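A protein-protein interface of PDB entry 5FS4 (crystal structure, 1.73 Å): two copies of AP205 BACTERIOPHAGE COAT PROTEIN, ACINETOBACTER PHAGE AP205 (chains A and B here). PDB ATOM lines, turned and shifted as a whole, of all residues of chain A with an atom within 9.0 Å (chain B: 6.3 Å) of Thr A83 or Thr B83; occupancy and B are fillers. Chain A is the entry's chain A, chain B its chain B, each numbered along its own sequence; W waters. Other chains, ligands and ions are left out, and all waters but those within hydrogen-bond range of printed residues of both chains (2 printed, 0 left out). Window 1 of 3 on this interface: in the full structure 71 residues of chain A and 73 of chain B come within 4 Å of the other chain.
The backbone carbonyl oxygen (O) of Arg A82 sits at hydrogen-bond distance from the backbone NH (N) of Val B84 (2.8 Å).
The side-chain hydroxyl (OG1) of Thr A83 sits at hydrogen-bond distance from a ring nitrogen (NE2) of His B102.
A ring nitrogen (NE2) of His A102 sits at hydrogen-bond distance from the side-chain hydroxyl (OG1) of Thr B83, at 2.8 Å.
The side-chain hydroxyl of Ser A55 lies within hydrogen-bond range of a ring nitrogen (ND1) of His B102.
The backbone NH (N) of Val A84 is in hydrogen-bond range of the backbone carbonyl oxygen (O) of Arg B82 (2.8 Å).
The side-chain carboxylate (OD1) of Asp A107 lies within hydrogen-bond range of the indole nitrogen (NE1) of Trp B99 (2.8 Å).
OG1 of Thr A83 sits at hydrogen-bond distance from OG1 of Thr B83, at 2.9 Å.
N of Gly B51 sits at hydrogen-bond distance from O of Ile B85 (2.8 Å).
N of Tyr B53 sits at hydrogen-bond distance from O of Thr B83, 2.7 Å away.
OE1 of Gln A52 sits at hydrogen-bond distance from NH2 of Arg A82, 2.8 Å away.
The backbone NH (N) of Tyr A53 lies within hydrogen-bond range of the backbone carbonyl oxygen (O) of Thr A83.
The backbone carbonyl oxygen of Ile A81 lies within hydrogen-bond range of the backbone NH of Ser A55 (2.9 Å).
Among the printed residues, pairs that only touch across the chains: Phe A30 with Val B106 (3.9 Å), Tyr A53 with His B102 (3.4 Å), Tyr A53 with Val B106 (3.7 Å), Ser A80 with Val B84 (3.8 Å), Ser A80 with Ile B85 (3.7 Å), Ile A81 with Thr B83 (3.7 Å), Ile A81 with Val B84 (3.4 Å), Ile A81 with Trp B99 (3.4 Å), Ile A81 with His B102 (3.5 Å), Arg A82 with Arg B82 (3.6 Å), Arg A82 with Thr B83 (3.2 Å), Thr A83 with Arg B82 (3.2 Å), Val A84 with Ile B81 (3.3 Å), Ile A85 with Ile B81 (3.9 Å), Trp A99 with Ile B81 (3.4 Å), Trp A99 with Val B106 (3.5 Å), His A102 with Tyr B53 (3.4 Å), His A102 with Ile B81 (3.4 Å), Val A106 with Tyr B53 (3.5 Å), Val A106 with Trp B99 (3.3 Å), Phe A110 with Tyr B53 (3.7 Å), Phe A110 with Ile B85 (3.8 Å) and Phe A110 with Trp B99 (3.7 Å).
Of the printed residues of chain B, Arg A82 touches Arg B82 (3.6 Å), Thr B83 (3.2 Å) and Val B84 (2.8 Å).
Thr A83 touches just these residues of chain B: Arg B82, Thr B83 and His B102.
Printed residues of chain B within 4 Å of Ile A85: Ile B81 (3.9 Å).
Gln B52 touches none of the printed residues of chain A.
Of chain A, only Ile A81, Arg A82, Thr A83 and His A102 come within 4 Å of Thr B83.
Printed residues of chain A within 4 Å of Trp B99: Ile A81, Val A106, Asp A107 and Phe A110.
The nearest residue of chain B that does not touch Thr A83 is Ile B81 (4.1 Å).
The nearest residue of chain A that does not touch Thr B83 is Trp A99 (4.5 Å).
The nearest printed residue of chain B that does not touch Ser A80 is His B102 (6.7 Å).
Printed residues of chain A that touch a printed residue of chain B: Phe A30, Tyr A53, Ser A55, Ser A80, Ile A81, Arg A82, Thr A83, Val A84, Ile A85, Trp A99, His A102, Val A106, Asp A107 and Phe A110.
Hydrophobic or aromatic side chains of chain A within 4 Å of the printed part of chain B: Phe A30, Tyr A53, Ile A81, Val A84, Ile A85, Trp A99, His A102, Val A106 and Phe A110.
Along chain A the printed residues that touch a printed residue of chain B span positions 30 to 110.
Ile A81 touches Val B84, and with the chains exchanged Val A84 touches Ile B81.
Ile A81 touches His B102, and with the chains exchanged His A102 touches Ile B81.
Arg B82 touches its own counterpart, Arg A82.
Thr A83 touches His B102, and with the chains exchanged His A102 touches Thr B83.
Positions printed for both chains: 51, 52, 53, 54, 81, 82, 83, 84, 85, 99, 102 and 106.
Water W2 bridges O of Val B84 (2.8 Å) and OG of Ser A80 (3.0 Å).
Water W1 bridges the guanidinium group (NE) of Arg B82 (3.0 Å) and the backbone carbonyl oxygen (O) of Arg A82 (3.0 Å).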
ATOM      1  N   PHE A  30      -6.525 -29.167  22.866  1.00  0.00           N
ATOM      2  CA  PHE A  30      -5.794 -27.972  23.316  1.00  0.00           C
ATOM      3  C   PHE A  30      -4.649 -27.750  22.380  1.00  0.00           C
ATOM      4  O   PHE A  30      -3.835 -28.639  22.174  1.00  0.00           O
ATOM      5  CB  PHE A  30      -5.272 -28.145  24.741  1.00  0.00           C
ATOM      6  CG  PHE A  30      -4.477 -26.972  25.255  1.00  0.00           C
ATOM      7  CD1 PHE A  30      -5.111 -25.865  25.736  1.00  0.00           C
ATOM      8  CD2 PHE A  30      -3.046 -27.029  25.315  1.00  0.00           C
ATOM      9  CE1 PHE A  30      -4.379 -24.816  26.278  1.00  0.00           C
ATOM     10  CE2 PHE A  30      -2.319 -25.936  25.811  1.00  0.00           C
ATOM     11  CZ  PHE A  30      -2.999 -24.844  26.280  1.00  0.00           C
ATOM     12  N   SER A  31      -4.542 -26.548  21.830  1.00  0.00           N
ATOM     13  CA  SER A  31      -3.480 -26.293  20.888  1.00  0.00           C
ATOM     14  C   SER A  31      -2.663 -25.067  21.301  1.00  0.00           C
ATOM     15  O   SER A  31      -3.214 -24.105  21.885  1.00  0.00           O
ATOM     16  CB  SER A  31      -4.060 -26.078  19.489  1.00  0.00           C
ATOM     17  OG  SER A  31      -4.671 -24.819  19.396  1.00  0.00           O
ATOM     18  N   ALA A  32      -1.356 -25.094  20.972  1.00  0.00           N
ATOM     19  CA  ALA A  32      -0.498 -23.947  21.314  1.00  0.00           C
ATOM     20  C   ALA A  32       0.274 -23.547  20.053  1.00  0.00           C
ATOM     21  O   ALA A  32       0.810 -24.400  19.440  1.00  0.00           O
ATOM     22  CB  ALA A  32       0.406 -24.318  22.482  1.00  0.00           C
ATOM     23  N   SER A  33       0.215 -22.258  19.641  1.00  0.00           N
ATOM     24  CA  SER A  33       0.873 -21.839  18.438  1.00  0.00           C
ATOM     25  C   SER A  33       1.606 -20.564  18.757  1.00  0.00           C
ATOM     26  O   SER A  33       1.038 -19.671  19.340  1.00  0.00           O
ATOM     27  CB  SER A  33      -0.135 -21.587  17.361  1.00  0.00           C
ATOM     28  OG  SER A  33       0.563 -21.107  16.194  1.00  0.00           O
ATOM     29  N   LEU A  34       2.866 -20.487  18.378  1.00  0.00           N
ATOM     30  CA  LEU A  34       3.734 -19.424  18.856  1.00  0.00           C
ATOM     31  C   LEU A  34       4.297 -18.704  17.659  1.00  0.00           C
ATOM     32  O   LEU A  34       4.610 -19.322  16.646  1.00  0.00           O
ATOM     33  CB  LEU A  34       4.880 -20.052  19.698  1.00  0.00           C
ATOM     34  CG  LEU A  34       4.530 -20.936  20.921  1.00  0.00           C
ATOM     35  CD1 LEU A  34       5.803 -21.283  21.647  1.00  0.00           C
ATOM     36  CD2 LEU A  34       3.537 -20.325  21.873  1.00  0.00           C
ATOM     37  N   SER A  50       4.067 -13.989  20.378  1.00  0.00           N
ATOM     38  CA  SER A  50       2.603 -14.013  20.522  1.00  0.00           C
ATOM     39  C   SER A  50       2.239 -15.469  20.644  1.00  0.00           C
ATOM     40  O   SER A  50       2.556 -16.236  19.718  1.00  0.00           O
ATOM     41  CB  SER A  50       1.946 -13.394  19.309  1.00  0.00           C
ATOM     42  OG  SER A  50       0.540 -13.361  19.449  1.00  0.00           O
ATOM     43  N   GLY A  51       1.660 -15.860  21.787  1.00  0.00           N
ATOM     44  CA  GLY A  51       1.326 -17.281  22.072  1.00  0.00           C
ATOM     45  C   GLY A  51      -0.172 -17.441  22.023  1.00  0.00           C
ATOM     46  O   GLY A  51      -0.863 -16.732  22.706  1.00  0.00           O
ATOM     47  N   GLN A  52      -0.683 -18.327  21.172  1.00  0.00           N
ATOM     48  CA  GLN A  52      -2.128 -18.518  20.999  1.00  0.00           C
ATOM     49  C   GLN A  52      -2.506 -19.899  21.519  1.00  0.00           C
ATOM     50  O   GLN A  52      -1.950 -20.897  21.051  1.00  0.00           O
ATOM     51  CB  GLN A  52      -2.509 -18.416  19.538  1.00  0.00           C
ATOM     52  CG  GLN A  52      -4.004 -18.472  19.302  1.00  0.00           C
ATOM     53  CD  GLN A  52      -4.333 -18.529  17.799  1.00  0.00           C
ATOM     54  OE1 GLN A  52      -4.932 -17.620  17.224  1.00  0.00           O
ATOM     55  NE2 GLN A  52      -3.912 -19.598  17.176  1.00  0.00           N
ATOM     56  N   TYR A  53      -3.362 -19.926  22.533  1.00  0.00           N
ATOM     57  CA  TYR A  53      -3.690 -21.140  23.287  1.00  0.00           C
ATOM     58  C   TYR A  53      -5.220 -21.347  23.167  1.00  0.00           C
ATOM     59  O   TYR A  53      -5.955 -20.516  23.603  1.00  0.00           O
ATOM     60  CB  TYR A  53      -3.286 -20.940  24.748  1.00  0.00           C
ATOM     61  CG  TYR A  53      -1.768 -20.602  24.949  1.00  0.00           C
ATOM     62  CD1 TYR A  53      -0.829 -21.617  25.031  1.00  0.00           C
ATOM     63  CD2 TYR A  53      -1.330 -19.311  25.039  1.00  0.00           C
ATOM     64  CE1 TYR A  53       0.537 -21.358  25.293  1.00  0.00           C
ATOM     65  CE2 TYR A  53       0.028 -19.009  25.226  1.00  0.00           C
ATOM     66  CZ  TYR A  53       0.980 -20.031  25.321  1.00  0.00           C
ATOM     67  OH  TYR A  53       2.321 -19.743  25.504  1.00  0.00           O
ATOM     68  N   VAL A  54      -5.674 -22.516  22.678  1.00  0.00           N
ATOM     69  CA  VAL A  54      -7.072 -22.720  22.336  1.00  0.00           C
ATOM     70  C   VAL A  54      -7.507 -24.071  22.862  1.00  0.00           C
ATOM     71  O   VAL A  54      -6.905 -25.077  22.530  1.00  0.00           O
ATOM     72  CB  VAL A  54      -7.374 -22.704  20.822  1.00  0.00           C
ATOM     73  CG1 VAL A  54      -8.886 -22.810  20.545  1.00  0.00           C
ATOM     74  CG2 VAL A  54      -6.792 -21.446  20.192  1.00  0.00           C
ATOM     75  N   SER A  55      -8.557 -24.015  23.658  1.00  0.00           N
ATOM     76  CA  SER A  55      -9.189 -25.170  24.264  1.00  0.00           C
ATOM     77  C   SER A  55     -10.522 -25.356  23.611  1.00  0.00           C
ATOM     78  O   SER A  55     -11.271 -24.409  23.483  1.00  0.00           O
ATOM     79  CB  SER A  55      -9.405 -24.911  25.744  1.00  0.00           C
ATOM     80  OG  SER A  55      -8.153 -24.817  26.363  1.00  0.00           O
ATOM     81  N   SER A  80     -15.365 -23.172  23.721  1.00  0.00           N
ATOM     82  CA  SER A  80     -14.014 -22.847  23.300  1.00  0.00           C
ATOM     83  C   SER A  80     -13.508 -21.695  24.103  1.00  0.00           C
ATOM     84  O   SER A  80     -14.251 -20.765  24.465  1.00  0.00           O
ATOM     85  CB  SER A  80     -13.878 -22.605  21.797  1.00  0.00           C
ATOM     86  OG  SER A  80     -14.489 -21.418  21.358  1.00  0.00           O
ATOM     87  N   ILE A  81     -12.216 -21.791  24.396  1.00  0.00           N
ATOM     88  CA  ILE A  81     -11.539 -20.740  25.131  1.00  0.00           C
ATOM     89  C   ILE A  81     -10.237 -20.454  24.358  1.00  0.00           C
ATOM     90  O   ILE A  81      -9.507 -21.371  24.138  1.00  0.00           O
ATOM     91  CB  ILE A  81     -11.251 -21.069  26.590  1.00  0.00           C
ATOM     92  CG1 ILE A  81     -12.558 -21.503  27.259  1.00  0.00           C
ATOM     93  CG2 ILE A  81     -10.532 -19.836  27.222  1.00  0.00           C
ATOM     94  CD1 ILE A  81     -12.539 -21.753  28.738  1.00  0.00           C
ATOM     95  N   ARG A  82     -10.017 -19.192  23.938  1.00  0.00           N
ATOM     96  CA  ARG A  82      -8.823 -18.804  23.159  1.00  0.00           C
ATOM     97  C   ARG A  82      -8.117 -17.681  23.878  1.00  0.00           C
ATOM     98  O   ARG A  82      -8.734 -16.646  24.159  1.00  0.00           O
ATOM     99  CB  ARG A  82      -9.187 -18.333  21.774  1.00  0.00           C
ATOM    100  CG  ARG A  82     -10.114 -19.262  21.029  1.00  0.00           C
ATOM    101  CD  ARG A  82     -10.546 -18.648  19.695  1.00  0.00           C
ATOM    102  NE  ARG A  82      -9.316 -18.330  18.949  1.00  0.00           N
ATOM    103  CZ  ARG A  82      -8.670 -19.128  18.090  1.00  0.00           C
ATOM    104  NH1 ARG A  82      -9.144 -20.336  17.755  1.00  0.00           N
ATOM    105  NH2 ARG A  82      -7.522 -18.691  17.540  1.00  0.00           N
ATOM    106  N   THR A  83      -6.837 -17.906  24.201  1.00  0.00           N
ATOM    107  CA  THR A  83      -6.056 -16.911  24.880  1.00  0.00           C
ATOM    108  C   THR A  83      -4.870 -16.590  23.996  1.00  0.00           C
ATOM    109  O   THR A  83      -4.148 -17.482  23.566  1.00  0.00           O
ATOM    110  CB  THR A  83      -5.519 -17.387  26.246  1.00  0.00           C
ATOM    111  OG1 THR A  83      -6.580 -17.492  27.173  1.00  0.00           O
ATOM    112  CG2 THR A  83      -4.549 -16.347  26.793  1.00  0.00           C
ATOM    113  N   VAL A  84      -4.613 -15.300  23.836  1.00  0.00           N
ATOM    114  CA  VAL A  84      -3.407 -14.876  23.172  1.00  0.00           C
ATOM    115  C   VAL A  84      -2.615 -14.073  24.136  1.00  0.00           C
ATOM    116  O   VAL A  84      -3.152 -13.083  24.643  1.00  0.00           O
ATOM    117  CB  VAL A  84      -3.702 -14.045  21.897  1.00  0.00           C
ATOM    118  CG1 VAL A  84      -2.422 -13.558  21.262  1.00  0.00           C
ATOM    119  CG2 VAL A  84      -4.488 -14.871  20.905  1.00  0.00           C
ATOM    120  N   ILE A  85      -1.345 -14.449  24.315  1.00  0.00           N
ATOM    121  CA  ILE A  85      -0.409 -13.685  25.195  1.00  0.00           C
ATOM    122  C   ILE A  85       0.667 -13.122  24.317  1.00  0.00           C
ATOM    123  O   ILE A  85       1.298 -13.854  23.569  1.00  0.00           O
ATOM    124  CB  ILE A  85       0.233 -14.592  26.228  1.00  0.00           C
ATOM    125  CG1 ILE A  85      -0.827 -15.000  27.238  1.00  0.00           C
ATOM    126  CG2 ILE A  85       1.382 -13.910  26.954  1.00  0.00           C
ATOM    127  CD1 ILE A  85      -0.433 -16.181  28.118  1.00  0.00           C
ATOM    128  N   SER A  86       0.893 -11.812  24.399  1.00  0.00           N
ATOM    129  CA  SER A  86       1.786 -11.171  23.436  1.00  0.00           C
ATOM    130  C   SER A  86       2.663 -10.147  24.150  1.00  0.00           C
ATOM    131  O   SER A  86       2.216  -9.118  24.675  1.00  0.00           O
ATOM    132  CB  SER A  86       1.031 -10.612  22.220  1.00  0.00           C
ATOM    133  OG  SER A  86       1.864  -9.906  21.303  1.00  0.00           O
ATOM    134  N   TRP A  99      -0.054 -12.242  33.147  1.00  0.00           N
ATOM    135  CA  TRP A  99      -0.910 -13.435  32.992  1.00  0.00           C
ATOM    136  C   TRP A  99      -1.599 -13.823  34.329  1.00  0.00           C
ATOM    137  O   TRP A  99      -2.800 -14.094  34.364  1.00  0.00           O
ATOM    138  CB  TRP A  99      -0.079 -14.559  32.459  1.00  0.00           C
ATOM    139  CG  TRP A  99      -0.746 -15.913  32.466  1.00  0.00           C
ATOM    140  CD1 TRP A  99      -0.241 -17.053  33.049  1.00  0.00           C
ATOM    141  CD2 TRP A  99      -1.986 -16.291  31.833  1.00  0.00           C
ATOM    142  NE1 TRP A  99      -1.072 -18.106  32.815  1.00  0.00           N
ATOM    143  CE2 TRP A  99      -2.155 -17.672  32.071  1.00  0.00           C
ATOM    144  CE3 TRP A  99      -2.974 -15.604  31.049  1.00  0.00           C
ATOM    145  CZ2 TRP A  99      -3.281 -18.378  31.606  1.00  0.00           C
ATOM    146  CZ3 TRP A  99      -4.052 -16.321  30.560  1.00  0.00           C
ATOM    147  CH2 TRP A  99      -4.216 -17.685  30.856  1.00  0.00           C
ATOM    148  N   HIS A 102      -4.380 -11.213  34.845  1.00  0.00           N
ATOM    149  CA  HIS A 102      -5.395 -11.505  33.828  1.00  0.00           C
ATOM    150  C   HIS A 102      -6.289 -12.608  34.269  1.00  0.00           C
ATOM    151  O   HIS A 102      -7.495 -12.450  34.281  1.00  0.00           O
ATOM    152  CB  HIS A 102      -4.742 -11.862  32.485  1.00  0.00           C
ATOM    153  CG  HIS A 102      -5.717 -12.119  31.379  1.00  0.00           C
ATOM    154  ND1 HIS A 102      -6.249 -11.103  30.627  1.00  0.00           N
ATOM    155  CD2 HIS A 102      -6.228 -13.270  30.873  1.00  0.00           C
ATOM    156  CE1 HIS A 102      -7.056 -11.608  29.708  1.00  0.00           C
ATOM    157  NE2 HIS A 102      -7.091 -12.917  29.863  1.00  0.00           N
ATOM    158  N   LYS A 103      -5.710 -13.732  34.684  1.00  0.00           N
ATOM    159  CA  LYS A 103      -6.555 -14.818  35.236  1.00  0.00           C
ATOM    160  C   LYS A 103      -7.402 -14.387  36.410  1.00  0.00           C
ATOM    161  O   LYS A 103      -8.519 -14.827  36.564  1.00  0.00           O
ATOM    162  CB  LYS A 103      -5.733 -16.025  35.678  1.00  0.00           C
ATOM    163  CG  LYS A 103      -5.077 -16.743  34.532  1.00  0.00           C
ATOM    164  CD  LYS A 103      -4.137 -17.859  35.015  1.00  0.00           C
ATOM    165  CE  LYS A 103      -2.838 -17.414  35.743  1.00  0.00           C
ATOM    166  NZ  LYS A 103      -2.038 -18.635  36.145  1.00  0.00           N
ATOM    167  N   VAL A 106     -10.256 -12.046  35.012  1.00  0.00           N
ATOM    168  CA  VAL A 106     -11.209 -12.923  34.386  1.00  0.00           C
ATOM    169  C   VAL A 106     -11.998 -13.790  35.393  1.00  0.00           C
ATOM    170  O   VAL A 106     -13.244 -13.942  35.290  1.00  0.00           O
ATOM    171  CB  VAL A 106     -10.525 -13.736  33.268  1.00  0.00           C
ATOM    172  CG1 VAL A 106     -11.520 -14.768  32.716  1.00  0.00           C
ATOM    173  CG2 VAL A 106     -10.014 -12.790  32.158  1.00  0.00           C
ATOM    174  N   ASP A 107     -11.304 -14.370  36.391  1.00  0.00           N
ATOM    175  CA  ASP A 107     -11.992 -15.121  37.443  1.00  0.00           C
ATOM    176  C   ASP A 107     -13.072 -14.307  38.107  1.00  0.00           C
ATOM    177  O   ASP A 107     -14.166 -14.811  38.363  1.00  0.00           O
ATOM    178  CB  ASP A 107     -11.013 -15.567  38.548  1.00  0.00           C
ATOM    179  CG  ASP A 107     -10.129 -16.749  38.151  1.00  0.00           C
ATOM    180  OD1 ASP A 107     -10.416 -17.428  37.140  1.00  0.00           O
ATOM    181  OD2 ASP A 107      -9.097 -16.966  38.839  1.00  0.00           O
ATOM    182  N   PHE A 110     -16.079 -13.929  35.359  1.00  0.00           N
ATOM    183  CA  PHE A 110     -16.614 -15.149  34.769  1.00  0.00           C
ATOM    184  C   PHE A 110     -16.658 -16.371  35.700  1.00  0.00           C
ATOM    185  O   PHE A 110     -17.615 -17.159  35.690  1.00  0.00           O
ATOM    186  CB  PHE A 110     -15.740 -15.510  33.566  1.00  0.00           C
ATOM    187  CG  PHE A 110     -16.054 -16.849  32.986  1.00  0.00           C
ATOM    188  CD1 PHE A 110     -17.080 -16.987  32.073  1.00  0.00           C
ATOM    189  CD2 PHE A 110     -15.263 -17.958  33.291  1.00  0.00           C
ATOM    190  CE1 PHE A 110     -17.393 -18.187  31.497  1.00  0.00           C
ATOM    191  CE2 PHE A 110     -15.629 -19.217  32.770  1.00  0.00           C
ATOM    192  CZ  PHE A 110     -16.681 -19.319  31.839  1.00  0.00           C
ATOM    193  N   GLY B  51     -17.553 -13.924  25.603  1.00  0.00           N
ATOM    194  CA  GLY B  51     -16.929 -12.874  26.395  1.00  0.00           C
ATOM    195  C   GLY B  51     -15.484 -12.674  26.053  1.00  0.00           C
ATOM    196  O   GLY B  51     -14.708 -13.618  26.022  1.00  0.00           O
ATOM    197  N   GLN B  52     -15.098 -11.419  25.860  1.00  0.00           N
ATOM    198  CA  GLN B  52     -13.727 -11.089  25.409  1.00  0.00           C
ATOM    199  C   GLN B  52     -13.140 -10.277  26.508  1.00  0.00           C
ATOM    200  O   GLN B  52     -13.707  -9.235  26.831  1.00  0.00           O
ATOM    201  CB  GLN B  52     -13.739 -10.235  24.159  1.00  0.00           C
ATOM    202  CG  GLN B  52     -12.359  -9.970  23.606  1.00  0.00           C
ATOM    203  CD  GLN B  52     -12.353  -8.924  22.530  1.00  0.00           C
ATOM    204  OE1 GLN B  52     -12.276  -9.241  21.358  1.00  0.00           O
ATOM    205  NE2 GLN B  52     -12.469  -7.650  22.941  1.00  0.00           N
ATOM    206  N   TYR B  53     -12.004 -10.721  27.028  1.00  0.00           N
ATOM    207  CA  TYR B  53     -11.334 -10.104  28.195  1.00  0.00           C
ATOM    208  C   TYR B  53      -9.935  -9.712  27.762  1.00  0.00           C
ATOM    209  O   TYR B  53      -9.185 -10.561  27.333  1.00  0.00           O
ATOM    210  CB  TYR B  53     -11.259 -11.108  29.350  1.00  0.00           C
ATOM    211  CG  TYR B  53     -12.577 -11.657  29.753  1.00  0.00           C
ATOM    212  CD1 TYR B  53     -13.358 -10.970  30.698  1.00  0.00           C
ATOM    213  CD2 TYR B  53     -13.113 -12.805  29.164  1.00  0.00           C
ATOM    214  CE1 TYR B  53     -14.621 -11.446  31.060  1.00  0.00           C
ATOM    215  CE2 TYR B  53     -14.412 -13.249  29.481  1.00  0.00           C
ATOM    216  CZ  TYR B  53     -15.165 -12.566  30.437  1.00  0.00           C
ATOM    217  OH  TYR B  53     -16.395 -13.104  30.770  1.00  0.00           O
ATOM    218  N   VAL B  54      -9.569  -8.441  27.872  1.00  0.00           N
ATOM    219  CA  VAL B  54      -8.287  -7.925  27.337  1.00  0.00           C
ATOM    220  C   VAL B  54      -7.499  -7.119  28.399  1.00  0.00           C
ATOM    221  O   VAL B  54      -8.024  -6.235  29.073  1.00  0.00           O
ATOM    222  CB  VAL B  54      -8.475  -7.039  26.049  1.00  0.00           C
ATOM    223  CG1 VAL B  54      -7.136  -6.634  25.526  1.00  0.00           C
ATOM    224  CG2 VAL B  54      -9.247  -7.758  24.970  1.00  0.00           C
ATOM    225  N   ILE B  81      -2.762  -9.310  26.739  1.00  0.00           N
ATOM    226  CA  ILE B  81      -3.353 -10.634  26.914  1.00  0.00           C
ATOM    227  C   ILE B  81      -4.831 -10.569  26.639  1.00  0.00           C
ATOM    228  O   ILE B  81      -5.543  -9.777  27.288  1.00  0.00           O
ATOM    229  CB  ILE B  81      -3.067 -11.250  28.317  1.00  0.00           C
ATOM    230  CG1 ILE B  81      -1.549 -11.224  28.621  1.00  0.00           C
ATOM    231  CG2 ILE B  81      -3.699 -12.643  28.359  1.00  0.00           C
ATOM    232  CD1 ILE B  81      -1.156 -11.846  29.943  1.00  0.00           C
ATOM    233  N   ARG B  82      -5.296 -11.418  25.713  1.00  0.00           N
ATOM    234  CA  ARG B  82      -6.704 -11.466  25.347  1.00  0.00           C
ATOM    235  C   ARG B  82      -7.243 -12.880  25.583  1.00  0.00           C
ATOM    236  O   ARG B  82      -6.683 -13.823  25.094  1.00  0.00           O
ATOM    237  CB  ARG B  82      -6.910 -11.067  23.860  1.00  0.00           C
ATOM    238  CG  ARG B  82      -8.372 -11.165  23.483  1.00  0.00           C
ATOM    239  CD  ARG B  82      -8.635 -10.796  22.068  1.00  0.00           C
ATOM    240  NE  ARG B  82      -8.012 -11.751  21.168  1.00  0.00           N
ATOM    241  CZ  ARG B  82      -7.451 -11.429  19.994  1.00  0.00           C
ATOM    242  NH1 ARG B  82      -7.330 -10.165  19.573  1.00  0.00           N
ATOM    243  NH2 ARG B  82      -6.953 -12.386  19.250  1.00  0.00           N
ATOM    244  N   THR B  83      -8.373 -13.004  26.252  1.00  0.00           N
ATOM    245  CA  THR B  83      -9.033 -14.333  26.333  1.00  0.00           C
ATOM    246  C   THR B  83     -10.431 -14.169  25.837  1.00  0.00           C
ATOM    247  O   THR B  83     -11.125 -13.126  26.116  1.00  0.00           O
ATOM    248  CB  THR B  83      -9.082 -14.916  27.779  1.00  0.00           C
ATOM    249  OG1 THR B  83      -7.769 -15.116  28.278  1.00  0.00           O
ATOM    250  CG2 THR B  83      -9.925 -16.279  27.908  1.00  0.00           C
ATOM    251  N   VAL B  84     -10.889 -15.148  25.061  1.00  0.00           N
ATOM    252  CA  VAL B  84     -12.257 -15.105  24.574  1.00  0.00           C
ATOM    253  C   VAL B  84     -12.878 -16.435  24.949  1.00  0.00           C
ATOM    254  O   VAL B  84     -12.318 -17.494  24.565  1.00  0.00           O
ATOM    255  CB  VAL B  84     -12.424 -14.953  23.034  1.00  0.00           C
ATOM    256  CG1 VAL B  84     -13.929 -14.925  22.704  1.00  0.00           C
ATOM    257  CG2 VAL B  84     -11.767 -13.680  22.572  1.00  0.00           C
ATOM    258  N   ILE B  85     -13.933 -16.368  25.771  1.00  0.00           N
ATOM    259  CA  ILE B  85     -14.644 -17.547  26.213  1.00  0.00           C
ATOM    260  C   ILE B  85     -15.994 -17.625  25.526  1.00  0.00           C
ATOM    261  O   ILE B  85     -16.802 -16.669  25.627  1.00  0.00           O
ATOM    262  CB  ILE B  85     -14.872 -17.476  27.698  1.00  0.00           C
ATOM    263  CG1 ILE B  85     -13.512 -17.412  28.429  1.00  0.00           C
ATOM    264  CG2 ILE B  85     -15.727 -18.633  28.164  1.00  0.00           C
ATOM    265  CD1 ILE B  85     -13.613 -17.327  29.931  1.00  0.00           C
ATOM    266  N   TRP B  99     -12.524 -23.475  31.727  1.00  0.00           N
ATOM    267  CA  TRP B  99     -11.662 -22.340  32.116  1.00  0.00           C
ATOM    268  C   TRP B  99     -10.623 -22.780  33.132  1.00  0.00           C
ATOM    269  O   TRP B  99      -9.440 -22.457  32.972  1.00  0.00           O
ATOM    270  CB  TRP B  99     -12.524 -21.145  32.612  1.00  0.00           C
ATOM    271  CG  TRP B  99     -11.745 -19.974  33.178  1.00  0.00           C
ATOM    272  CD1 TRP B  99     -11.905 -19.456  34.438  1.00  0.00           C
ATOM    273  CD2 TRP B  99     -10.733 -19.148  32.542  1.00  0.00           C
ATOM    274  NE1 TRP B  99     -11.073 -18.383  34.615  1.00  0.00           N
ATOM    275  CE2 TRP B  99     -10.312 -18.202  33.497  1.00  0.00           C
ATOM    276  CE3 TRP B  99     -10.077 -19.174  31.298  1.00  0.00           C
ATOM    277  CZ2 TRP B  99      -9.309 -17.217  33.211  1.00  0.00           C
ATOM    278  CZ3 TRP B  99      -9.111 -18.247  31.034  1.00  0.00           C
ATOM    279  CH2 TRP B  99      -8.746 -17.261  31.980  1.00  0.00           C
ATOM    280  N   HIS B 102      -8.095 -24.893  31.115  1.00  0.00           N
ATOM    281  CA  HIS B 102      -7.347 -24.067  30.157  1.00  0.00           C
ATOM    282  C   HIS B 102      -6.218 -23.270  30.849  1.00  0.00           C
ATOM    283  O   HIS B 102      -5.121 -23.152  30.312  1.00  0.00           O
ATOM    284  CB  HIS B 102      -8.382 -23.182  29.398  1.00  0.00           C
ATOM    285  CG  HIS B 102      -7.769 -22.097  28.560  1.00  0.00           C
ATOM    286  ND1 HIS B 102      -7.561 -22.245  27.198  1.00  0.00           N
ATOM    287  CD2 HIS B 102      -7.377 -20.842  28.862  1.00  0.00           C
ATOM    288  CE1 HIS B 102      -7.117 -21.108  26.697  1.00  0.00           C
ATOM    289  NE2 HIS B 102      -6.939 -20.260  27.695  1.00  0.00           N
ATOM    290  N   VAL B 106      -2.307 -23.653  29.966  1.00  0.00           N
ATOM    291  CA  VAL B 106      -1.523 -22.512  29.616  1.00  0.00           C
ATOM    292  C   VAL B 106      -0.372 -22.332  30.617  1.00  0.00           C
ATOM    293  O   VAL B 106       0.761 -22.092  30.200  1.00  0.00           O
ATOM    294  CB  VAL B 106      -2.342 -21.204  29.499  1.00  0.00           C
ATOM    295  CG1 VAL B 106      -1.372 -20.056  29.213  1.00  0.00           C
ATOM    296  CG2 VAL B 106      -3.429 -21.295  28.416  1.00  0.00           C
HETATM  297  O   HOH W   1      -8.003 -14.569  22.128  1.00  0.00           O
HETATM  298  O   HOH W   2     -13.334 -18.861  22.318  1.00  0.00           O
